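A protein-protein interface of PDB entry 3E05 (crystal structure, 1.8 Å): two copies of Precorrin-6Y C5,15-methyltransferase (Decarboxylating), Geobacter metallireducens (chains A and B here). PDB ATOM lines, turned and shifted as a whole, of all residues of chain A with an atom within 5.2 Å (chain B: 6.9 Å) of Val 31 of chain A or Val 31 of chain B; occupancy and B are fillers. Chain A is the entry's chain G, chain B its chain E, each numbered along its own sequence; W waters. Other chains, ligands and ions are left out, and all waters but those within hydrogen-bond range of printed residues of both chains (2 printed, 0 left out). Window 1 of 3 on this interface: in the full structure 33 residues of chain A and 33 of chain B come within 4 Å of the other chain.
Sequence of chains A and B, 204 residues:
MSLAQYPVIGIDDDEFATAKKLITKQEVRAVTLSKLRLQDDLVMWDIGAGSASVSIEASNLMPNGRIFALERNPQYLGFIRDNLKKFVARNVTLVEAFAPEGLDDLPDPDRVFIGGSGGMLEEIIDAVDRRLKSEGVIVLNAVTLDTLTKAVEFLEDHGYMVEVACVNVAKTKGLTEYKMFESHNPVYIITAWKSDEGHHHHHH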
ATOM      1  N   GLU A  27     -26.248 -10.405   8.549  1.00  0.00           N
ATOM      2  CA  GLU A  27     -27.269 -10.341   9.603  1.00  0.00           C
ATOM      3  C   GLU A  27     -26.675 -10.589  10.979  1.00  0.00           C
ATOM      4  O   GLU A  27     -26.855  -9.785  11.896  1.00  0.00           O
ATOM      5  CB  GLU A  27     -28.408 -11.343   9.338  1.00  0.00           C
ATOM      6  CG  GLU A  27     -29.162 -11.090   8.028  1.00  0.00           C
ATOM      7  CD  GLU A  27     -28.493 -11.678   6.775  1.00  0.00           C
ATOM      8  OE1 GLU A  27     -27.449 -12.366   6.858  1.00  0.00           O
ATOM      9  OE2 GLU A  27     -29.021 -11.423   5.679  1.00  0.00           O
ATOM     10  N   VAL A  28     -25.964 -11.704  11.094  1.00  0.00           N
ATOM     11  CA  VAL A  28     -25.271 -12.113  12.310  1.00  0.00           C
ATOM     12  C   VAL A  28     -24.183 -11.090  12.676  1.00  0.00           C
ATOM     13  O   VAL A  28     -23.979 -10.782  13.860  1.00  0.00           O
ATOM     14  CB  VAL A  28     -24.703 -13.551  12.132  1.00  0.00           C
ATOM     15  CG1 VAL A  28     -23.559 -13.833  13.076  1.00  0.00           C
ATOM     16  CG2 VAL A  28     -25.837 -14.603  12.303  1.00  0.00           C
ATOM     17  N   ARG A  29     -23.494 -10.575  11.668  1.00  0.00           N
ATOM     18  CA  ARG A  29     -22.529  -9.484  11.875  1.00  0.00           C
ATOM     19  C   ARG A  29     -23.187  -8.269  12.552  1.00  0.00           C
ATOM     20  O   ARG A  29     -22.616  -7.691  13.456  1.00  0.00           O
ATOM     21  CB  ARG A  29     -21.878  -9.071  10.561  1.00  0.00           C
ATOM     22  CG  ARG A  29     -20.619  -8.197  10.705  1.00  0.00           C
ATOM     23  CD  ARG A  29     -20.251  -7.580   9.351  1.00  0.00           C
ATOM     24  NE  ARG A  29     -20.238  -8.574   8.281  1.00  0.00           N
ATOM     25  CZ  ARG A  29     -20.806  -8.432   7.087  1.00  0.00           C
ATOM     26  NH1 ARG A  29     -21.458  -7.325   6.761  1.00  0.00           N
ATOM     27  NH2 ARG A  29     -20.741  -9.431   6.221  1.00  0.00           N
ATOM     28  N   ALA A  30     -24.375  -7.878  12.102  1.00  0.00           N
ATOM     29  CA  ALA A  30     -25.095  -6.757  12.718  1.00  0.00           C
ATOM     30  C   ALA A  30     -25.444  -7.012  14.185  1.00  0.00           C
ATOM     31  O   ALA A  30     -25.271  -6.134  15.039  1.00  0.00           O
ATOM     32  CB  ALA A  30     -26.352  -6.443  11.923  1.00  0.00           C
ATOM     33  N   VAL A  31     -25.946  -8.210  14.480  1.00  0.00           N
ATOM     34  CA  VAL A  31     -26.254  -8.600  15.855  1.00  0.00           C
ATOM     35  C   VAL A  31     -24.973  -8.636  16.685  1.00  0.00           C
ATOM     36  O   VAL A  31     -24.954  -8.211  17.845  1.00  0.00           O
ATOM     37  CB  VAL A  31     -26.996  -9.969  15.924  1.00  0.00           C
ATOM     38  CG1 VAL A  31     -27.431 -10.277  17.363  1.00  0.00           C
ATOM     39  CG2 VAL A  31     -28.207  -9.950  14.996  1.00  0.00           C
ATOM     40  N   THR A  32     -23.894  -9.115  16.074  1.00  0.00           N
ATOM     41  CA  THR A  32     -22.594  -9.161  16.760  1.00  0.00           C
ATOM     42  C   THR A  32     -22.094  -7.740  17.130  1.00  0.00           C
ATOM     43  O   THR A  32     -21.721  -7.488  18.283  1.00  0.00           O
ATOM     44  CB  THR A  32     -21.560  -9.930  15.889  1.00  0.00           C
ATOM     45  OG1 THR A  32     -21.986 -11.293  15.714  1.00  0.00           O
ATOM     46  CG2 THR A  32     -20.176  -9.915  16.515  1.00  0.00           C
ATOM     47  N   LEU A  33     -22.130  -6.812  16.171  1.00  0.00           N
ATOM     48  CA  LEU A  33     -21.779  -5.395  16.440  1.00  0.00           C
ATOM     49  C   LEU A  33     -22.670  -4.798  17.525  1.00  0.00           C
ATOM     50  O   LEU A  33     -22.189  -4.086  18.402  1.00  0.00           O
ATOM     51  CB  LEU A  33     -21.870  -4.547  15.171  1.00  0.00           C
ATOM     52  CG  LEU A  33     -20.926  -4.977  14.051  1.00  0.00           C
ATOM     53  CD1 LEU A  33     -21.356  -4.328  12.775  1.00  0.00           C
ATOM     54  CD2 LEU A  33     -19.474  -4.665  14.422  1.00  0.00           C
ATOM     55  N   SER A  34     -23.963  -5.122  17.463  1.00  0.00           N
ATOM     56  CA  SER A  34     -24.937  -4.722  18.483  1.00  0.00           C
ATOM     57  C   SER A  34     -24.540  -5.216  19.869  1.00  0.00           C
ATOM     58  O   SER A  34     -24.579  -4.455  20.842  1.00  0.00           O
ATOM     59  CB  SER A  34     -26.320  -5.257  18.116  1.00  0.00           C
ATOM     60  OG  SER A  34     -27.327  -4.558  18.797  1.00  0.00           O
ATOM     61  N   LYS A  35     -24.107  -6.473  19.953  1.00  0.00           N
ATOM     62  CA  LYS A  35     -23.738  -7.072  21.241  1.00  0.00           C
ATOM     63  C   LYS A  35     -22.411  -6.544  21.779  1.00  0.00           C
ATOM     64  O   LYS A  35     -22.169  -6.568  22.997  1.00  0.00           O
ATOM     65  CB  LYS A  35     -23.715  -8.602  21.155  1.00  0.00           C
ATOM     66  CG  LYS A  35     -25.102  -9.271  20.851  1.00  0.00           C
ATOM     67  CD  LYS A  35     -26.113  -9.121  21.966  1.00  0.00           C
ATOM     68  CE  LYS A  35     -27.419  -9.796  21.585  1.00  0.00           C
ATOM     69  NZ  LYS A  35     -28.452  -9.625  22.631  1.00  0.00           N
ATOM     70  N   LEU A  36     -21.561  -6.079  20.866  1.00  0.00           N
ATOM     71  CA  LEU A  36     -20.253  -5.524  21.230  1.00  0.00           C
ATOM     72  C   LEU A  36     -20.340  -4.180  21.952  1.00  0.00           C
ATOM     73  O   LEU A  36     -19.352  -3.755  22.538  1.00  0.00           O
ATOM     74  CB  LEU A  36     -19.330  -5.426  20.006  1.00  0.00           C
ATOM     75  CG  LEU A  36     -18.627  -6.746  19.637  1.00  0.00           C
ATOM     76  CD1 LEU A  36     -18.120  -6.761  18.208  1.00  0.00           C
ATOM     77  CD2 LEU A  36     -17.503  -7.118  20.630  1.00  0.00           C
ATOM     78  N   VAL A 167     -28.911 -17.464  16.829  1.00  0.00           N
ATOM     79  CA  VAL A 167     -29.530 -16.727  15.742  1.00  0.00           C
ATOM     80  C   VAL A 167     -29.649 -17.614  14.500  1.00  0.00           C
ATOM     81  O   VAL A 167     -28.665 -18.101  13.955  1.00  0.00           O
ATOM     82  CB  VAL A 167     -28.814 -15.352  15.447  1.00  0.00           C
ATOM     83  CG1 VAL A 167     -29.461 -14.641  14.255  1.00  0.00           C
ATOM     84  CG2 VAL A 167     -28.866 -14.423  16.684  1.00  0.00           C
ATOM     85  N   ILE A 189     -24.202 -16.550  19.310  1.00  0.00           N
ATOM     86  CA  ILE A 189     -23.507 -15.293  19.638  1.00  0.00           C
ATOM     87  C   ILE A 189     -23.457 -15.224  21.151  1.00  0.00           C
ATOM     88  O   ILE A 189     -24.494 -15.114  21.817  1.00  0.00           O
ATOM     89  CB  ILE A 189     -24.230 -14.059  19.057  1.00  0.00           C
ATOM     90  CG1 ILE A 189     -24.387 -14.207  17.541  1.00  0.00           C
ATOM     91  CG2 ILE A 189     -23.435 -12.774  19.359  1.00  0.00           C
ATOM     92  CD1 ILE A 189     -25.209 -13.121  16.905  1.00  0.00           C
ATOM     93  N   ILE B   9     -25.129   1.379  18.489  1.00  0.00           N
ATOM     94  CA  ILE B   9     -26.265   0.457  18.312  1.00  0.00           C
ATOM     95  C   ILE B   9     -26.151  -0.572  19.436  1.00  0.00           C
ATOM     96  O   ILE B   9     -25.083  -0.726  20.027  1.00  0.00           O
ATOM     97  CB  ILE B   9     -26.314  -0.220  16.888  1.00  0.00           C
ATOM     98  CG1 ILE B   9     -25.129  -1.177  16.688  1.00  0.00           C
ATOM     99  CG2 ILE B   9     -26.432   0.837  15.753  1.00  0.00           C
ATOM    100  CD1 ILE B   9     -25.224  -2.110  15.465  1.00  0.00           C
ATOM    101  N   LYS B  25     -37.053  -5.317  19.177  1.00  0.00           N
ATOM    102  CA  LYS B  25     -36.049  -5.808  20.137  1.00  0.00           C
ATOM    103  C   LYS B  25     -34.648  -5.715  19.540  1.00  0.00           C
ATOM    104  O   LYS B  25     -34.518  -5.679  18.334  1.00  0.00           O
ATOM    105  CB  LYS B  25     -36.324  -7.262  20.527  1.00  0.00           C
ATOM    106  CG  LYS B  25     -37.692  -7.487  21.168  1.00  0.00           C
ATOM    107  CD  LYS B  25     -37.864  -8.927  21.580  1.00  0.00           C
ATOM    108  CE  LYS B  25     -39.343  -9.258  21.855  1.00  0.00           C
ATOM    109  NZ  LYS B  25     -39.770  -8.861  23.242  1.00  0.00           N
ATOM    110  N   GLN B  26     -33.630  -5.700  20.401  1.00  0.00           N
ATOM    111  CA  GLN B  26     -32.246  -5.343  20.049  1.00  0.00           C
ATOM    112  C   GLN B  26     -31.637  -6.053  18.821  1.00  0.00           C
ATOM    113  O   GLN B  26     -31.096  -5.410  17.913  1.00  0.00           O
ATOM    114  CB  GLN B  26     -31.338  -5.580  21.258  1.00  0.00           C
ATOM    115  CG  GLN B  26     -29.876  -5.229  21.004  1.00  0.00           C
ATOM    116  CD  GLN B  26     -28.905  -5.961  21.923  1.00  0.00           C
ATOM    117  OE1 GLN B  26     -29.293  -6.538  22.937  1.00  0.00           O
ATOM    118  NE2 GLN B  26     -27.627  -5.935  21.562  1.00  0.00           N
ATOM    119  N   GLU B  27     -31.739  -7.372  18.794  1.00  0.00           N
ATOM    120  CA  GLU B  27     -31.095  -8.185  17.730  1.00  0.00           C
ATOM    121  C   GLU B  27     -31.762  -7.938  16.384  1.00  0.00           C
ATOM    122  O   GLU B  27     -31.092  -7.670  15.385  1.00  0.00           O
ATOM    123  CB  GLU B  27     -31.164  -9.668  18.080  1.00  0.00           C
ATOM    124  CG  GLU B  27     -30.547 -10.009  19.430  1.00  0.00           C
ATOM    125  CD  GLU B  27     -31.496  -9.842  20.628  1.00  0.00           C
ATOM    126  OE1 GLU B  27     -32.676  -9.395  20.482  1.00  0.00           O
ATOM    127  OE2 GLU B  27     -31.032 -10.172  21.731  1.00  0.00           O
ATOM    128  N   VAL B  28     -33.085  -8.000  16.383  1.00  0.00           N
ATOM    129  CA  VAL B  28     -33.886  -7.722  15.180  1.00  0.00           C
ATOM    130  C   VAL B  28     -33.685  -6.256  14.740  1.00  0.00           C
ATOM    131  O   VAL B  28     -33.578  -5.986  13.552  1.00  0.00           O
ATOM    132  CB  VAL B  28     -35.367  -8.101  15.415  1.00  0.00           C
ATOM    133  CG1 VAL B  28     -36.331  -7.349  14.473  1.00  0.00           C
ATOM    134  CG2 VAL B  28     -35.546  -9.622  15.273  1.00  0.00           C
ATOM    135  N   ARG B  29     -33.611  -5.340  15.713  1.00  0.00           N
ATOM    136  CA  ARG B  29     -33.338  -3.908  15.460  1.00  0.00           C
ATOM    137  C   ARG B  29     -32.026  -3.742  14.711  1.00  0.00           C
ATOM    138  O   ARG B  29     -31.968  -3.025  13.721  1.00  0.00           O
ATOM    139  CB  ARG B  29     -33.289  -3.124  16.787  1.00  0.00           C
ATOM    140  CG  ARG B  29     -33.276  -1.581  16.629  1.00  0.00           C
ATOM    141  CD  ARG B  29     -32.974  -0.861  17.976  1.00  0.00           C
ATOM    142  NE  ARG B  29     -33.769  -1.373  19.074  1.00  0.00           N
ATOM    143  CZ  ARG B  29     -33.305  -1.784  20.246  1.00  0.00           C
ATOM    144  NH1 ARG B  29     -32.008  -1.720  20.561  1.00  0.00           N
ATOM    145  NH2 ARG B  29     -34.166  -2.236  21.133  1.00  0.00           N
ATOM    146  N   ALA B  30     -30.980  -4.428  15.185  1.00  0.00           N
ATOM    147  CA  ALA B  30     -29.673  -4.447  14.513  1.00  0.00           C
ATOM    148  C   ALA B  30     -29.740  -4.929  13.050  1.00  0.00           C
ATOM    149  O   ALA B  30     -29.213  -4.270  12.162  1.00  0.00           O
ATOM    150  CB  ALA B  30     -28.682  -5.280  15.309  1.00  0.00           C
ATOM    151  N   VAL B  31     -30.460  -6.032  12.798  1.00  0.00           N
ATOM    152  CA  VAL B  31     -30.576  -6.558  11.441  1.00  0.00           C
ATOM    153  C   VAL B  31     -31.399  -5.582  10.604  1.00  0.00           C
ATOM    154  O   VAL B  31     -31.068  -5.319   9.456  1.00  0.00           O
ATOM    155  CB  VAL B  31     -31.196  -7.988  11.382  1.00  0.00           C
ATOM    156  CG1 VAL B  31     -31.213  -8.489   9.915  1.00  0.00           C
ATOM    157  CG2 VAL B  31     -30.428  -8.984  12.271  1.00  0.00           C
ATOM    158  N   THR B  32     -32.456  -5.027  11.189  1.00  0.00           N
ATOM    159  CA  THR B  32     -33.292  -4.041  10.478  1.00  0.00           C
ATOM    160  C   THR B  32     -32.445  -2.840  10.014  1.00  0.00           C
ATOM    161  O   THR B  32     -32.527  -2.417   8.861  1.00  0.00           O
ATOM    162  CB  THR B  32     -34.451  -3.582  11.391  1.00  0.00           C
ATOM    163  OG1 THR B  32     -35.260  -4.722  11.734  1.00  0.00           O
ATOM    164  CG2 THR B  32     -35.295  -2.550  10.719  1.00  0.00           C
ATOM    165  N   LEU B  33     -31.632  -2.310  10.923  1.00  0.00           N
ATOM    166  CA  LEU B  33     -30.713  -1.216  10.597  1.00  0.00           C
ATOM    167  C   LEU B  33     -29.729  -1.578   9.494  1.00  0.00           C
ATOM    168  O   LEU B  33     -29.480  -0.762   8.614  1.00  0.00           O
ATOM    169  CB  LEU B  33     -29.949  -0.769  11.837  1.00  0.00           C
ATOM    170  CG  LEU B  33     -30.785  -0.054  12.905  1.00  0.00           C
ATOM    171  CD1 LEU B  33     -29.970   0.016  14.163  1.00  0.00           C
ATOM    172  CD2 LEU B  33     -31.249   1.334  12.465  1.00  0.00           C
ATOM    173  N   SER B  34     -29.205  -2.804   9.546  1.00  0.00           N
ATOM    174  CA  SER B  34     -28.299  -3.323   8.533  1.00  0.00           C
ATOM    175  C   SER B  34     -28.959  -3.395   7.159  1.00  0.00           C
ATOM    176  O   SER B  34     -28.351  -3.058   6.149  1.00  0.00           O
ATOM    177  CB  SER B  34     -27.792  -4.696   8.973  1.00  0.00           C
ATOM    178  OG  SER B  34     -27.238  -5.411   7.902  1.00  0.00           O
ATOM    179  N   LYS B  35     -30.217  -3.833   7.133  1.00  0.00           N
ATOM    180  CA  LYS B  35     -30.935  -3.957   5.876  1.00  0.00           C
ATOM    181  C   LYS B  35     -31.299  -2.587   5.310  1.00  0.00           C
ATOM    182  O   LYS B  35     -31.423  -2.416   4.080  1.00  0.00           O
ATOM    183  CB  LYS B  35     -32.208  -4.791   6.042  1.00  0.00           C
ATOM    184  CG  LYS B  35     -31.987  -6.266   6.380  1.00  0.00           C
ATOM    185  CD  LYS B  35     -31.294  -7.043   5.255  1.00  0.00           C
ATOM    186  CE  LYS B  35     -30.883  -8.457   5.752  1.00  0.00           C
ATOM    187  NZ  LYS B  35     -30.213  -9.223   4.672  1.00  0.00           N
ATOM    188  N   LEU B  36     -31.431  -1.612   6.200  1.00  0.00           N
ATOM    189  CA  LEU B  36     -31.706  -0.236   5.783  1.00  0.00           C
ATOM    190  C   LEU B  36     -30.568   0.451   4.988  1.00  0.00           C
ATOM    191  O   LEU B  36     -30.781   1.543   4.460  1.00  0.00           O
ATOM    192  CB  LEU B  36     -32.134   0.602   6.998  1.00  0.00           C
ATOM    193  CG  LEU B  36     -33.617   0.530   7.370  1.00  0.00           C
ATOM    194  CD1 LEU B  36     -33.854   0.910   8.836  1.00  0.00           C
ATOM    195  CD2 LEU B  36     -34.462   1.398   6.433  1.00  0.00           C
ATOM    196  N   ARG B  37     -29.383  -0.172   4.910  1.00  0.00           N
ATOM    197  CA  ARG B  37     -28.265   0.296   4.044  1.00  0.00           C
ATOM    198  C   ARG B  37     -27.935   1.765   4.294  1.00  0.00           C
ATOM    199  O   ARG B  37     -27.874   2.578   3.352  1.00  0.00           O
ATOM    200  CB  ARG B  37     -28.607   0.133   2.552  1.00  0.00           C
ATOM    201  CG  ARG B  37     -27.871  -0.934   1.782  1.00  0.00           C
ATOM    202  CD  ARG B  37     -28.756  -2.128   1.552  1.00  0.00           C
ATOM    203  NE  ARG B  37     -28.366  -3.271   2.370  1.00  0.00           N
ATOM    204  CZ  ARG B  37     -29.157  -4.305   2.639  1.00  0.00           C
ATOM    205  NH1 ARG B  37     -30.404  -4.331   2.174  1.00  0.00           N
ATOM    206  NH2 ARG B  37     -28.706  -5.310   3.384  1.00  0.00           N
ATOM    207  N   VAL B 139     -37.756  -0.777   4.241  1.00  0.00           N
ATOM    208  CA  VAL B 139     -37.697  -1.953   5.137  1.00  0.00           C
ATOM    209  C   VAL B 139     -38.980  -2.025   5.991  1.00  0.00           C
ATOM    210  O   VAL B 139     -39.466  -1.016   6.517  1.00  0.00           O
ATOM    211  CB  VAL B 139     -36.396  -1.976   6.029  1.00  0.00           C
ATOM    212  CG1 VAL B 139     -36.407  -3.139   7.023  1.00  0.00           C
ATOM    213  CG2 VAL B 139     -35.111  -2.050   5.170  1.00  0.00           C
ATOM    214  N   ASN B 141     -41.022  -4.662   9.022  1.00  0.00           N
ATOM    215  CA  ASN B 141     -40.935  -5.832   9.885  1.00  0.00           C
ATOM    216  C   ASN B 141     -42.339  -6.370  10.044  1.00  0.00           C
ATOM    217  O   ASN B 141     -43.225  -5.653  10.489  1.00  0.00           O
ATOM    218  CB  ASN B 141     -40.329  -5.502  11.253  1.00  0.00           C
ATOM    219  CG  ASN B 141     -38.809  -5.300  11.215  1.00  0.00           C
ATOM    220  OD1 ASN B 141     -38.193  -5.085  12.254  1.00  0.00           O
ATOM    221  ND2 ASN B 141     -38.210  -5.385  10.048  1.00  0.00           N
ATOM    222  N   ALA B 165     -36.231 -11.798   4.891  1.00  0.00           N
ATOM    223  CA  ALA B 165     -35.378 -12.532   5.832  1.00  0.00           C
ATOM    224  C   ALA B 165     -36.160 -12.863   7.105  1.00  0.00           C
ATOM    225  O   ALA B 165     -36.649 -11.974   7.792  1.00  0.00           O
ATOM    226  CB  ALA B 165     -34.115 -11.726   6.176  1.00  0.00           C
ATOM    227  N   VAL B 167     -36.033 -14.024  10.819  1.00  0.00           N
ATOM    228  CA  VAL B 167     -35.001 -14.032  11.855  1.00  0.00           C
ATOM    229  C   VAL B 167     -35.585 -14.631  13.125  1.00  0.00           C
ATOM    230  O   VAL B 167     -36.585 -14.146  13.643  1.00  0.00           O
ATOM    231  CB  VAL B 167     -34.422 -12.615  12.151  1.00  0.00           C
ATOM    232  CG1 VAL B 167     -33.306 -12.705  13.218  1.00  0.00           C
ATOM    233  CG2 VAL B 167     -33.897 -12.002  10.895  1.00  0.00           C
ATOM    234  N   VAL B 169     -34.580 -15.814  16.980  1.00  0.00           N
ATOM    235  CA  VAL B 169     -33.599 -15.618  18.038  1.00  0.00           C
ATOM    236  C   VAL B 169     -34.022 -16.398  19.291  1.00  0.00           C
ATOM    237  O   VAL B 169     -35.123 -16.208  19.786  1.00  0.00           O
ATOM    238  CB  VAL B 169     -33.462 -14.094  18.407  1.00  0.00           C
ATOM    239  CG1 VAL B 169     -32.466 -13.899  19.539  1.00  0.00           C
ATOM    240  CG2 VAL B 169     -33.092 -13.225  17.166  1.00  0.00           C
ATOM    241  N   ILE B 189     -38.156  -9.661   8.127  1.00  0.00           N
ATOM    242  CA  ILE B 189     -37.629  -8.324   7.719  1.00  0.00           C
ATOM    243  C   ILE B 189     -37.636  -8.281   6.212  1.00  0.00           C
ATOM    244  O   ILE B 189     -36.916  -9.017   5.556  1.00  0.00           O
ATOM    245  CB  ILE B 189     -36.207  -8.062   8.268  1.00  0.00           C
ATOM    246  CG1 ILE B 189     -36.213  -8.247   9.781  1.00  0.00           C
ATOM    247  CG2 ILE B 189     -35.704  -6.657   7.822  1.00  0.00           C
ATOM    248  CD1 ILE B 189     -34.831  -8.278  10.462  1.00  0.00           C
ATOM    249  N   THR B 191     -37.047  -6.310   2.789  1.00  0.00           N
ATOM    250  CA  THR B 191     -36.251  -5.204   2.221  1.00  0.00           C
ATOM    251  C   THR B 191     -36.559  -5.045   0.739  1.00  0.00           C
ATOM    252  O   THR B 191     -36.480  -6.009  -0.018  1.00  0.00           O
ATOM    253  CB  THR B 191     -34.752  -5.425   2.474  1.00  0.00           C
ATOM    254  OG1 THR B 191     -34.566  -5.658   3.863  1.00  0.00           O
ATOM    255  CG2 THR B 191     -33.892  -4.206   2.068  1.00  0.00           C
HETATM  256  O   HOH W   1     -22.701  -1.556  19.218  1.00  0.00           O
HETATM  257  O   HOH W   2     -29.416  -3.019  17.959  1.00  0.00           O
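Val 31 of chain A touches just these residues of chain B: Glu 27 (3.7 Å) and Val 31 (3.6 Å). Of the printed residues of chain A, Val 31 of chain B touches Glu 27 (3.7 Å) and Val 31 (3.6 Å). Of the printed residues of chain A, Gln 26 of chain B touches Ser 34 and Lys 35. Of the printed residues of chain A, Ala 30 of chain B touches Ala 30 (3.5 Å) and Ser 34 (3.7 Å). Of the printed residues of chain B, Ser 34 of chain A touches Ile 9, Gln 26 and Ala 30. Arg 29 of chain B touches none of the printed residues of chain A. Val 139 of chain B touches none of the printed residues of chain A. The nearest residue of chain B that does not touch Val 31 of chain A is Ala 30 of chain B (4.1 Å). The nearest residue of chain A that does not touch Val 31 of chain B is Ala 30 of chain A (4.2 Å). The nearest printed residue of chain A that does not touch Ser 34 of chain B is Glu 27 of chain A (5.1 Å).
Among the printed residues, merely in contact across the chains: Glu 27 of chain A with Val 31 of chain B, Ala 30 of chain A with Ala 30 of chain B, Ala 30 of chain A with Ser 34 of chain B, Val 31 of chain A with Glu 27 of chain B, Val 31 of chain A with Val 31 of chain B, Ser 34 of chain A with Ile 9 of chain B and Ser 34 of chain A with Ala 30 of chain B.
Printed residues of chain B that touch a printed residue of chain A: Ile 9, Gln 26, Glu 27, Ala 30, Val 31, Ser 34 and Lys 35. Hydrophobic or aromatic side chains of chain B within 4 Å of the printed part of chain A: Ile 9, Ala 30 and Val 31. Among the printed residues, 11 pairs touch across the chains. Among the printed residues, Asp or Glu carboxylates within 4 Å of a Lys or Arg side-chain nitrogen of the other chain: Glu 27 of chain A with Lys 35 of chain B and Lys 35 of chain A with Glu 27 of chain B.
The backbone carbonyl oxygen (O) of Lys 35 of chain B lies within hydrogen-bond range of the guanidinium group (NH1) of Arg 37 of chain B (2.9 Å).
Glu 27 of chain A touches Val 31 of chain B, and with the chains exchanged Val 31 of chain A touches Glu 27 of chain B. Ala 30 of chain A touches its own counterpart, Ala 30 of chain B. Ala 30 of chain A touches Ser 34 of chain B, and with the chains exchanged Ser 34 of chain A touches Ala 30 of chain B. Val 31 of chain A touches its own counterpart, Val 31 of chain B. Positions printed for both chains: 27, 28, 29, 30, 31, 32, 33, 34, 35, 36, 167 and 189. Of the 11 pairs that touch across the chains among the printed residues, 8 have their exchanged pair printed and touching as well.
OE1 of Gln 26 of chain B sits at hydrogen-bond distance from NZ of Lys 35 of chain A. OE2 of Glu 27 of chain A lies within salt-bridge range of NZ of Lys 35 of chain B (2.7 Å). NE2 of Gln 26 of chain B lies within hydrogen-bond range of OG of Ser 34 of chain A (3.1 Å). OE2 of Glu 27 of chain B lies within salt-bridge range of NZ of Lys 35 of chain A (2.8 Å).
Water W1 bridges O of Ile 9 of chain B (2.6 Å) and O of Leu 33 of chain A (2.7 Å). Water W2 lies within hydrogen-bond range of the side-chain hydroxyl (OG) of Ser 34 of chain A (2.7 Å), the backbone carbonyl oxygen (O) of Gln 26 of chain B (2.9 Å) and the backbone NH (N) of Ala 30 of chain B (3.5 Å).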
